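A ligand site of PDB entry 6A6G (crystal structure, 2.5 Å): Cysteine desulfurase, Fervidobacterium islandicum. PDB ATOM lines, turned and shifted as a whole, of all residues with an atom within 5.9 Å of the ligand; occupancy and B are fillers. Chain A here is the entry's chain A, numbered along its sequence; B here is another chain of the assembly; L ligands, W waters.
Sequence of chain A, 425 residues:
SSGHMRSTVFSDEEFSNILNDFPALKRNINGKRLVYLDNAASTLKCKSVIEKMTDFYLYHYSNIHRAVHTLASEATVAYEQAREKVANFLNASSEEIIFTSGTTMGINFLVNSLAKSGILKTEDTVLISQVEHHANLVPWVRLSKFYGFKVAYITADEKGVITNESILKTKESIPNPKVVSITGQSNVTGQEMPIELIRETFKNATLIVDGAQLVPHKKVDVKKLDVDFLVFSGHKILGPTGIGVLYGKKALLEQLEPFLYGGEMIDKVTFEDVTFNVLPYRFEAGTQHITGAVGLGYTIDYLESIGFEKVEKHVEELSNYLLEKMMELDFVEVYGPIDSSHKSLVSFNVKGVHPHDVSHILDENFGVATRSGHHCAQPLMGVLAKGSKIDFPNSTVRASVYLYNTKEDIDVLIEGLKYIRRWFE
A carbon (C5) of the ligand is bonded to the side-chain amino group of Lys 236.
The side-chain carboxylate (OD2) of Asp 210 sits at hydrogen-bond distance from a nitrogen (N1) of the ligand (2.5 Å).
An oxygen (O5) of the ligand is in hydrogen-bond range of the side-chain hydroxyl of Ser 233 (2.6 Å).
The side-chain amide nitrogen (NE2) of Gln 213 is in hydrogen-bond range of an oxygen (O1) of the ligand (2.7 Å).
An oxygen (O4) of the ligand is in hydrogen-bond range of the backbone NH (N) of Thr 287 of chain B (2.9 Å).
O4 of the ligand lies within hydrogen-bond range of OG1 of Thr 287 of chain B, at 2.7 Å.
O3 of the ligand lies within hydrogen-bond range of N of Thr 104 (2.9 Å).
An oxygen (O3) of the ligand lies within hydrogen-bond range of the side-chain hydroxyl (OG1) of Thr 104 (2.7 Å).
A ring nitrogen (NE2) of His 235 sits at hydrogen-bond distance from an oxygen (O5) of the ligand (2.8 Å).
N of Ala 212 lies within hydrogen-bond range of OD1 of Asp 210, at 3.1 Å.
OE1 of Gln 185 lies close to O of Gln 213 (3.2 Å).
O of Ala 40 lies within hydrogen-bond range of NE2 of Gln 213 (3.1 Å).
A ring nitrogen (NE2) of His 235 lies within hydrogen-bond range of the side-chain hydroxyl (OG1) of Thr 287 of chain B, at 3.5 Å.
The side-chain hydroxyl of Thr 287 of chain B sits at hydrogen-bond distance from the side-chain amide nitrogen of Asn 63 of chain B (3.0 Å).
ND1 of His 133 is in hydrogen-bond range of N of Ala 135.
NE of Arg 398 is in hydrogen-bond range of O of Asn 187, 3.2 Å away.
O of Gln 185 lies within hydrogen-bond range of OG1 of Thr 183 (2.7 Å).
Thr 103 touches the ligand (N to O3, 3.5 Å).
His 133 touches the ligand (CB to N1, 3.5 Å).
CB of Ala 135 touches C7 of the ligand, at 3.9 Å.
Thr 183 touches the ligand.
Gln 185 touches the ligand.
CB of Asn 187 touches O1 of the ligand (3.6 Å).
CB of Ala 212 touches C3 of the ligand (3.6 Å).
Gly 286 of chain B touches the ligand.
Within 4 Å of the ligand: Thr 103, Thr 104, His 133, Ala 135, Thr 183, Gln 185, Asn 187, Asp 210, Ala 212, Gln 213, Ser 233, His 235, Lys 236, Gly 286 of chain B and Thr 287 of chain B.
Along chain A the residues within 4 Å of the ligand span positions 103 to 236.
The nearest printed residue that does not touch the ligand is Gly 102 (4.2 Å).
Water W4 bridges an oxygen (O4) of the ligand (2.6 Å) and the side-chain carboxylate (OE1) of Glu 264 of chain B (3.2 Å).
Water W1 bridges an oxygen (O3) of the ligand and the backbone carbonyl oxygen of Thr 287 of chain B.
Water W3 bridges NE2 of His 133 (3.2 Å) and NZ of Lys 236 (3.5 Å).
Water W5 lies within hydrogen-bond range of the backbone carbonyl oxygen (O) of Ser 101, an oxygen (O5) of the ligand and the backbone carbonyl oxygen (O) of Thr 287 of chain B.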
ATOM      1  N   ALA A  40      -3.706 -21.076  -8.634  1.00  0.00           N
ATOM      2  CA  ALA A  40      -3.830 -19.656  -8.307  1.00  0.00           C
ATOM      3  C   ALA A  40      -2.851 -18.728  -9.060  1.00  0.00           C
ATOM      4  O   ALA A  40      -2.972 -17.510  -8.966  1.00  0.00           O
ATOM      5  CB  ALA A  40      -3.646 -19.462  -6.806  1.00  0.00           C
ATOM      6  N   ALA A  41      -1.847 -19.307  -9.709  1.00  0.00           N
ATOM      7  CA  ALA A  41      -0.913 -18.550 -10.559  1.00  0.00           C
ATOM      8  C   ALA A  41      -1.311 -18.663 -11.994  1.00  0.00           C
ATOM      9  O   ALA A  41      -1.154 -17.725 -12.752  1.00  0.00           O
ATOM     10  CB  ALA A  41       0.517 -19.058 -10.385  1.00  0.00           C
ATOM     11  N   SER A 101      -5.151  -7.328 -22.027  1.00  0.00           N
ATOM     12  CA  SER A 101      -4.075  -8.316 -22.000  1.00  0.00           C
ATOM     13  C   SER A 101      -4.059  -9.098 -20.677  1.00  0.00           C
ATOM     14  O   SER A 101      -3.306 -10.090 -20.547  1.00  0.00           O
ATOM     15  CB  SER A 101      -2.727  -7.619 -22.166  1.00  0.00           C
ATOM     16  OG  SER A 101      -2.484  -6.784 -21.068  1.00  0.00           O
ATOM     17  N   GLY A 102      -4.865  -8.652 -19.703  1.00  0.00           N
ATOM     18  CA  GLY A 102      -4.890  -9.221 -18.377  1.00  0.00           C
ATOM     19  C   GLY A 102      -5.579  -8.364 -17.315  1.00  0.00           C
ATOM     20  O   GLY A 102      -5.944  -7.190 -17.525  1.00  0.00           O
ATOM     21  N   THR A 103      -5.768  -8.974 -16.150  1.00  0.00           N
ATOM     22  CA  THR A 103      -6.226  -8.237 -14.997  1.00  0.00           C
ATOM     23  C   THR A 103      -5.334  -7.016 -14.750  1.00  0.00           C
ATOM     24  O   THR A 103      -5.827  -5.904 -14.597  1.00  0.00           O
ATOM     25  CB  THR A 103      -6.231  -9.145 -13.793  1.00  0.00           C
ATOM     26  OG1 THR A 103      -7.149 -10.196 -14.035  1.00  0.00           O
ATOM     27  CG2 THR A 103      -6.648  -8.385 -12.543  1.00  0.00           C
ATOM     28  N   THR A 104      -4.026  -7.212 -14.766  1.00  0.00           N
ATOM     29  CA  THR A 104      -3.125  -6.115 -14.474  1.00  0.00           C
ATOM     30  C   THR A 104      -3.376  -4.922 -15.348  1.00  0.00           C
ATOM     31  O   THR A 104      -3.489  -3.818 -14.847  1.00  0.00           O
ATOM     32  CB  THR A 104      -1.634  -6.514 -14.592  1.00  0.00           C
ATOM     33  OG1 THR A 104      -1.361  -7.571 -13.675  1.00  0.00           O
ATOM     34  CG2 THR A 104      -0.784  -5.314 -14.214  1.00  0.00           C
ATOM     35  N   MET A 105      -3.453  -5.140 -16.646  1.00  0.00           N
ATOM     36  CA  MET A 105      -3.671  -4.024 -17.561  1.00  0.00           C
ATOM     37  C   MET A 105      -5.030  -3.390 -17.273  1.00  0.00           C
ATOM     38  O   MET A 105      -5.165  -2.210 -17.314  1.00  0.00           O
ATOM     39  CB  MET A 105      -3.543  -4.437 -19.037  1.00  0.00           C
ATOM     40  CG  MET A 105      -4.097  -3.371 -20.014  1.00  0.00           C
ATOM     41  SD  MET A 105      -4.129  -3.888 -21.758  1.00  0.00           S
ATOM     42  CE  MET A 105      -5.275  -2.703 -22.505  1.00  0.00           C
ATOM     43  N   ILE A 107      -6.647  -3.089 -14.504  1.00  0.00           N
ATOM     44  CA  ILE A 107      -6.539  -2.181 -13.340  1.00  0.00           C
ATOM     45  C   ILE A 107      -5.800  -0.898 -13.658  1.00  0.00           C
ATOM     46  O   ILE A 107      -6.238   0.152 -13.229  1.00  0.00           O
ATOM     47  CB  ILE A 107      -5.951  -2.861 -12.100  1.00  0.00           C
ATOM     48  CG1 ILE A 107      -7.016  -3.749 -11.491  1.00  0.00           C
ATOM     49  CG2 ILE A 107      -5.582  -1.853 -11.011  1.00  0.00           C
ATOM     50  CD1 ILE A 107      -6.424  -4.838 -10.654  1.00  0.00           C
ATOM     51  N   HIS A 133      -3.485  -8.012  -4.133  1.00  0.00           N
ATOM     52  CA  HIS A 133      -2.441  -8.379  -5.051  1.00  0.00           C
ATOM     53  C   HIS A 133      -1.782  -7.096  -5.576  1.00  0.00           C
ATOM     54  O   HIS A 133      -2.449  -6.035  -5.726  1.00  0.00           O
ATOM     55  CB  HIS A 133      -3.071  -9.164  -6.207  1.00  0.00           C
ATOM     56  CG  HIS A 133      -2.103  -9.813  -7.147  1.00  0.00           C
ATOM     57  ND1 HIS A 133      -1.323  -9.094  -8.034  1.00  0.00           N
ATOM     58  CD2 HIS A 133      -1.849 -11.121  -7.405  1.00  0.00           C
ATOM     59  CE1 HIS A 133      -0.633  -9.926  -8.791  1.00  0.00           C
ATOM     60  NE2 HIS A 133      -0.926 -11.165  -8.433  1.00  0.00           N
ATOM     61  N   ALA A 135      -1.207  -6.150  -8.363  1.00  0.00           N
ATOM     62  CA  ALA A 135      -1.911  -5.525  -9.470  1.00  0.00           C
ATOM     63  C   ALA A 135      -3.052  -4.580  -9.047  1.00  0.00           C
ATOM     64  O   ALA A 135      -3.412  -3.703  -9.818  1.00  0.00           O
ATOM     65  CB  ALA A 135      -2.436  -6.586 -10.426  1.00  0.00           C
ATOM     66  N   ASN A 136      -3.604  -4.762  -7.850  1.00  0.00           N
ATOM     67  CA  ASN A 136      -4.608  -3.858  -7.345  1.00  0.00           C
ATOM     68  C   ASN A 136      -4.114  -3.024  -6.169  1.00  0.00           C
ATOM     69  O   ASN A 136      -4.918  -2.560  -5.315  1.00  0.00           O
ATOM     70  CB  ASN A 136      -5.842  -4.609  -6.896  1.00  0.00           C
ATOM     71  CG  ASN A 136      -7.056  -3.713  -6.811  1.00  0.00           C
ATOM     72  OD1 ASN A 136      -7.162  -2.680  -7.507  1.00  0.00           O
ATOM     73  ND2 ASN A 136      -8.019  -4.123  -5.996  1.00  0.00           N
ATOM     74  N   THR A 183     -10.445  -6.910  -3.954  1.00  0.00           N
ATOM     75  CA  THR A 183     -10.403  -8.242  -4.544  1.00  0.00           C
ATOM     76  C   THR A 183     -11.689  -9.031  -4.281  1.00  0.00           C
ATOM     77  O   THR A 183     -12.278  -8.959  -3.196  1.00  0.00           O
ATOM     78  CB  THR A 183      -9.192  -9.050  -4.031  1.00  0.00           C
ATOM     79  OG1 THR A 183      -9.163 -10.317  -4.691  1.00  0.00           O
ATOM     80  CG2 THR A 183      -9.275  -9.265  -2.543  1.00  0.00           C
ATOM     81  N   GLN A 185     -11.575 -12.214  -4.315  1.00  0.00           N
ATOM     82  CA  GLN A 185     -10.992 -13.303  -3.521  1.00  0.00           C
ATOM     83  C   GLN A 185      -9.493 -13.152  -3.463  1.00  0.00           C
ATOM     84  O   GLN A 185      -8.860 -12.955  -4.510  1.00  0.00           O
ATOM     85  CB  GLN A 185     -11.334 -14.669  -4.134  1.00  0.00           C
ATOM     86  CG  GLN A 185     -10.660 -15.856  -3.469  1.00  0.00           C
ATOM     87  CD  GLN A 185     -11.088 -17.166  -4.096  1.00  0.00           C
ATOM     88  OE1 GLN A 185     -11.759 -17.187  -5.115  1.00  0.00           O
ATOM     89  NE2 GLN A 185     -10.718 -18.282  -3.465  1.00  0.00           N
ATOM     90  N   SER A 186      -8.913 -13.255  -2.251  1.00  0.00           N
ATOM     91  CA  SER A 186      -7.488 -13.032  -2.076  1.00  0.00           C
ATOM     92  C   SER A 186      -6.707 -14.196  -2.616  1.00  0.00           C
ATOM     93  O   SER A 186      -7.061 -15.327  -2.339  1.00  0.00           O
ATOM     94  CB  SER A 186      -7.110 -12.915  -0.600  1.00  0.00           C
ATOM     95  OG  SER A 186      -5.701 -13.103  -0.444  1.00  0.00           O
ATOM     96  N   ASN A 187      -5.606 -13.916  -3.293  1.00  0.00           N
ATOM     97  CA  ASN A 187      -4.756 -14.979  -3.821  1.00  0.00           C
ATOM     98  C   ASN A 187      -3.785 -15.533  -2.782  1.00  0.00           C
ATOM     99  O   ASN A 187      -3.032 -16.432  -3.095  1.00  0.00           O
ATOM    100  CB  ASN A 187      -3.978 -14.517  -5.062  1.00  0.00           C
ATOM    101  CG  ASN A 187      -2.840 -13.576  -4.731  1.00  0.00           C
ATOM    102  OD1 ASN A 187      -3.001 -12.656  -3.938  1.00  0.00           O
ATOM    103  ND2 ASN A 187      -1.684 -13.803  -5.338  1.00  0.00           N
ATOM    104  N   ASP A 210     -11.413  -6.866  -8.343  1.00  0.00           N
ATOM    105  CA  ASP A 210     -10.368  -7.661  -8.931  1.00  0.00           C
ATOM    106  C   ASP A 210     -10.857  -9.072  -8.800  1.00  0.00           C
ATOM    107  O   ASP A 210     -10.783  -9.664  -7.740  1.00  0.00           O
ATOM    108  CB  ASP A 210      -9.025  -7.442  -8.213  1.00  0.00           C
ATOM    109  CG  ASP A 210      -7.966  -8.401  -8.672  1.00  0.00           C
ATOM    110  OD1 ASP A 210      -8.265  -9.303  -9.512  1.00  0.00           O
ATOM    111  OD2 ASP A 210      -6.821  -8.275  -8.162  1.00  0.00           O
ATOM    112  N   ALA A 212      -9.817 -11.842 -10.450  1.00  0.00           N
ATOM    113  CA  ALA A 212      -8.924 -12.761 -11.156  1.00  0.00           C
ATOM    114  C   ALA A 212      -8.922 -14.174 -10.547  1.00  0.00           C
ATOM    115  O   ALA A 212      -8.750 -15.180 -11.232  1.00  0.00           O
ATOM    116  CB  ALA A 212      -7.517 -12.194 -11.172  1.00  0.00           C
ATOM    117  N   GLN A 213      -9.089 -14.205  -9.245  1.00  0.00           N
ATOM    118  CA  GLN A 213      -9.072 -15.436  -8.470  1.00  0.00           C
ATOM    119  C   GLN A 213     -10.498 -15.987  -8.260  1.00  0.00           C
ATOM    120  O   GLN A 213     -10.675 -17.169  -8.139  1.00  0.00           O
ATOM    121  CB  GLN A 213      -8.366 -15.132  -7.148  1.00  0.00           C
ATOM    122  CG  GLN A 213      -7.597 -16.273  -6.509  1.00  0.00           C
ATOM    123  CD  GLN A 213      -6.615 -16.990  -7.430  1.00  0.00           C
ATOM    124  OE1 GLN A 213      -6.721 -18.179  -7.568  1.00  0.00           O
ATOM    125  NE2 GLN A 213      -5.665 -16.274  -8.018  1.00  0.00           N
ATOM    126  N   SER A 233      -8.460 -12.438 -15.719  1.00  0.00           N
ATOM    127  CA  SER A 233      -7.498 -12.925 -16.715  1.00  0.00           C
ATOM    128  C   SER A 233      -7.901 -14.302 -17.240  1.00  0.00           C
ATOM    129  O   SER A 233      -8.255 -15.197 -16.469  1.00  0.00           O
ATOM    130  CB  SER A 233      -6.074 -13.041 -16.122  1.00  0.00           C
ATOM    131  OG  SER A 233      -5.562 -11.805 -15.652  1.00  0.00           O
ATOM    132  N   HIS A 235      -5.939 -16.626 -18.393  1.00  0.00           N
ATOM    133  CA  HIS A 235      -5.049 -17.777 -18.191  1.00  0.00           C
ATOM    134  C   HIS A 235      -5.357 -18.481 -16.881  1.00  0.00           C
ATOM    135  O   HIS A 235      -4.937 -19.609 -16.675  1.00  0.00           O
ATOM    136  CB  HIS A 235      -3.587 -17.373 -18.286  1.00  0.00           C
ATOM    137  CG  HIS A 235      -3.145 -16.450 -17.217  1.00  0.00           C
ATOM    138  ND1 HIS A 235      -2.556 -16.895 -16.065  1.00  0.00           N
ATOM    139  CD2 HIS A 235      -3.224 -15.090 -17.123  1.00  0.00           C
ATOM    140  CE1 HIS A 235      -2.292 -15.843 -15.298  1.00  0.00           C
ATOM    141  NE2 HIS A 235      -2.674 -14.745 -15.924  1.00  0.00           N
ATOM    142  N   LYS A 236      -6.105 -17.839 -16.007  1.00  0.00           N
ATOM    143  CA  LYS A 236      -6.546 -18.457 -14.730  1.00  0.00           C
ATOM    144  C   LYS A 236      -7.846 -19.300 -14.804  1.00  0.00           C
ATOM    145  O   LYS A 236      -8.232 -19.982 -13.843  1.00  0.00           O
ATOM    146  CB  LYS A 236      -6.654 -17.392 -13.667  1.00  0.00           C
ATOM    147  CG  LYS A 236      -5.323 -17.205 -12.992  1.00  0.00           C
ATOM    148  CD  LYS A 236      -5.159 -15.810 -12.477  1.00  0.00           C
ATOM    149  CE  LYS A 236      -3.867 -15.713 -11.691  1.00  0.00           C
ATOM    150  NZ  LYS A 236      -3.837 -14.461 -10.883  1.00  0.00           N
ATOM    151  N   ARG A 398       2.184 -21.885  -1.011  1.00  0.00           N
ATOM    152  CA  ARG A 398       0.773 -21.843  -1.313  1.00  0.00           C
ATOM    153  C   ARG A 398       0.372 -22.979  -2.198  1.00  0.00           C
ATOM    154  O   ARG A 398       0.951 -23.160  -3.231  1.00  0.00           O
ATOM    155  CB  ARG A 398       0.443 -20.507  -1.893  1.00  0.00           C
ATOM    156  CG  ARG A 398      -0.991 -20.275  -2.269  1.00  0.00           C
ATOM    157  CD  ARG A 398      -1.052 -20.109  -3.750  1.00  0.00           C
ATOM    158  NE  ARG A 398      -1.118 -18.734  -4.149  1.00  0.00           N
ATOM    159  CZ  ARG A 398      -0.751 -18.270  -5.329  1.00  0.00           C
ATOM    160  NH1 ARG A 398      -0.206 -19.043  -6.255  1.00  0.00           N
ATOM    161  NH2 ARG A 398      -0.937 -16.992  -5.593  1.00  0.00           N
ATOM    162  N   ASN B  63       2.914 -20.347 -15.189  1.00  0.00           N
ATOM    163  CA  ASN B  63       3.341 -18.954 -15.074  1.00  0.00           C
ATOM    164  C   ASN B  63       4.817 -18.938 -14.769  1.00  0.00           C
ATOM    165  O   ASN B  63       5.385 -19.977 -14.425  1.00  0.00           O
ATOM    166  CB  ASN B  63       2.602 -18.200 -13.951  1.00  0.00           C
ATOM    167  CG  ASN B  63       2.341 -16.761 -14.332  1.00  0.00           C
ATOM    168  OD1 ASN B  63       3.132 -16.147 -15.076  1.00  0.00           O
ATOM    169  ND2 ASN B  63       1.226 -16.199 -13.853  1.00  0.00           N
ATOM    170  N   GLU B 264       5.668  -8.703 -10.727  1.00  0.00           N
ATOM    171  CA  GLU B 264       6.827  -9.018 -11.569  1.00  0.00           C
ATOM    172  C   GLU B 264       7.795  -7.856 -11.723  1.00  0.00           C
ATOM    173  O   GLU B 264       8.994  -8.037 -11.574  1.00  0.00           O
ATOM    174  CB  GLU B 264       6.411  -9.661 -12.926  1.00  0.00           C
ATOM    175  CG  GLU B 264       6.122 -11.192 -12.859  1.00  0.00           C
ATOM    176  CD  GLU B 264       4.613 -11.557 -12.753  1.00  0.00           C
ATOM    177  OE1 GLU B 264       3.762 -10.637 -12.765  1.00  0.00           O
ATOM    178  OE2 GLU B 264       4.243 -12.766 -12.682  1.00  0.00           O
ATOM    179  N   ALA B 285       4.592  -5.675 -16.615  1.00  0.00           N
ATOM    180  CA  ALA B 285       3.722  -5.706 -15.433  1.00  0.00           C
ATOM    181  C   ALA B 285       2.773  -6.888 -15.595  1.00  0.00           C
ATOM    182  O   ALA B 285       2.149  -7.049 -16.648  1.00  0.00           O
ATOM    183  CB  ALA B 285       2.966  -4.401 -15.307  1.00  0.00           C
ATOM    184  N   GLY B 286       2.694  -7.727 -14.576  1.00  0.00           N
ATOM    185  CA  GLY B 286       1.798  -8.870 -14.584  1.00  0.00           C
ATOM    186  C   GLY B 286       2.171  -9.992 -15.543  1.00  0.00           C
ATOM    187  O   GLY B 286       3.202  -9.941 -16.205  1.00  0.00           O
ATOM    188  N   THR B 287       1.336 -11.023 -15.616  1.00  0.00           N
ATOM    189  CA  THR B 287       1.578 -12.146 -16.509  1.00  0.00           C
ATOM    190  C   THR B 287       1.529 -11.623 -17.945  1.00  0.00           C
ATOM    191  O   THR B 287       0.536 -11.068 -18.402  1.00  0.00           O
ATOM    192  CB  THR B 287       0.497 -13.218 -16.294  1.00  0.00           C
ATOM    193  OG1 THR B 287       0.387 -13.509 -14.899  1.00  0.00           O
ATOM    194  CG2 THR B 287       0.795 -14.506 -17.089  1.00  0.00           C
HETATM  195  N1  LIG L   1      -5.189 -10.124  -8.777  1.00  0.00           N
HETATM  196  C1  LIG L   1      -5.361 -11.349  -8.259  1.00  0.00           C
HETATM  197  C2  LIG L   1      -6.192 -11.504  -7.021  1.00  0.00           C
HETATM  198  C3  LIG L   1      -4.720 -12.502  -8.913  1.00  0.00           C
HETATM  199  O1  LIG L   1      -4.866 -13.771  -8.466  1.00  0.00           O
HETATM  200  C4  LIG L   1      -3.928 -12.224 -10.133  1.00  0.00           C
HETATM  201  C5  LIG L   1      -3.282 -13.317 -10.867  1.00  0.00           C
HETATM  202  C6  LIG L   1      -3.803 -10.842 -10.591  1.00  0.00           C
HETATM  203  C7  LIG L   1      -4.448  -9.844  -9.861  1.00  0.00           C
HETATM  204  C8  LIG L   1      -2.988 -10.529 -11.831  1.00  0.00           C
HETATM  205  O2  LIG L   1      -3.231 -11.370 -12.949  1.00  0.00           O
HETATM  206  P1  LIG L   1      -2.364 -11.153 -14.289  1.00  0.00           P
HETATM  207  O3  LIG L   1      -2.637  -9.728 -14.687  1.00  0.00           O
HETATM  208  O4  LIG L   1      -0.934 -11.427 -13.879  1.00  0.00           O
HETATM  209  O5  LIG L   1      -2.966 -12.067 -15.305  1.00  0.00           O
HETATM  210  O   HOH W   1      -1.784  -9.704 -17.291  1.00  0.00           O
HETATM  211  O   HOH W   2      -6.370 -10.487  -3.739  1.00  0.00           O
HETATM  212  O   HOH W   3      -0.489 -13.838 -10.159  1.00  0.00           O
HETATM  213  O   HOH W   4       0.668 -10.857 -11.853  1.00  0.00           O
HETATM  214  O   HOH W   5      -2.844 -11.929 -18.507  1.00  0.00           O
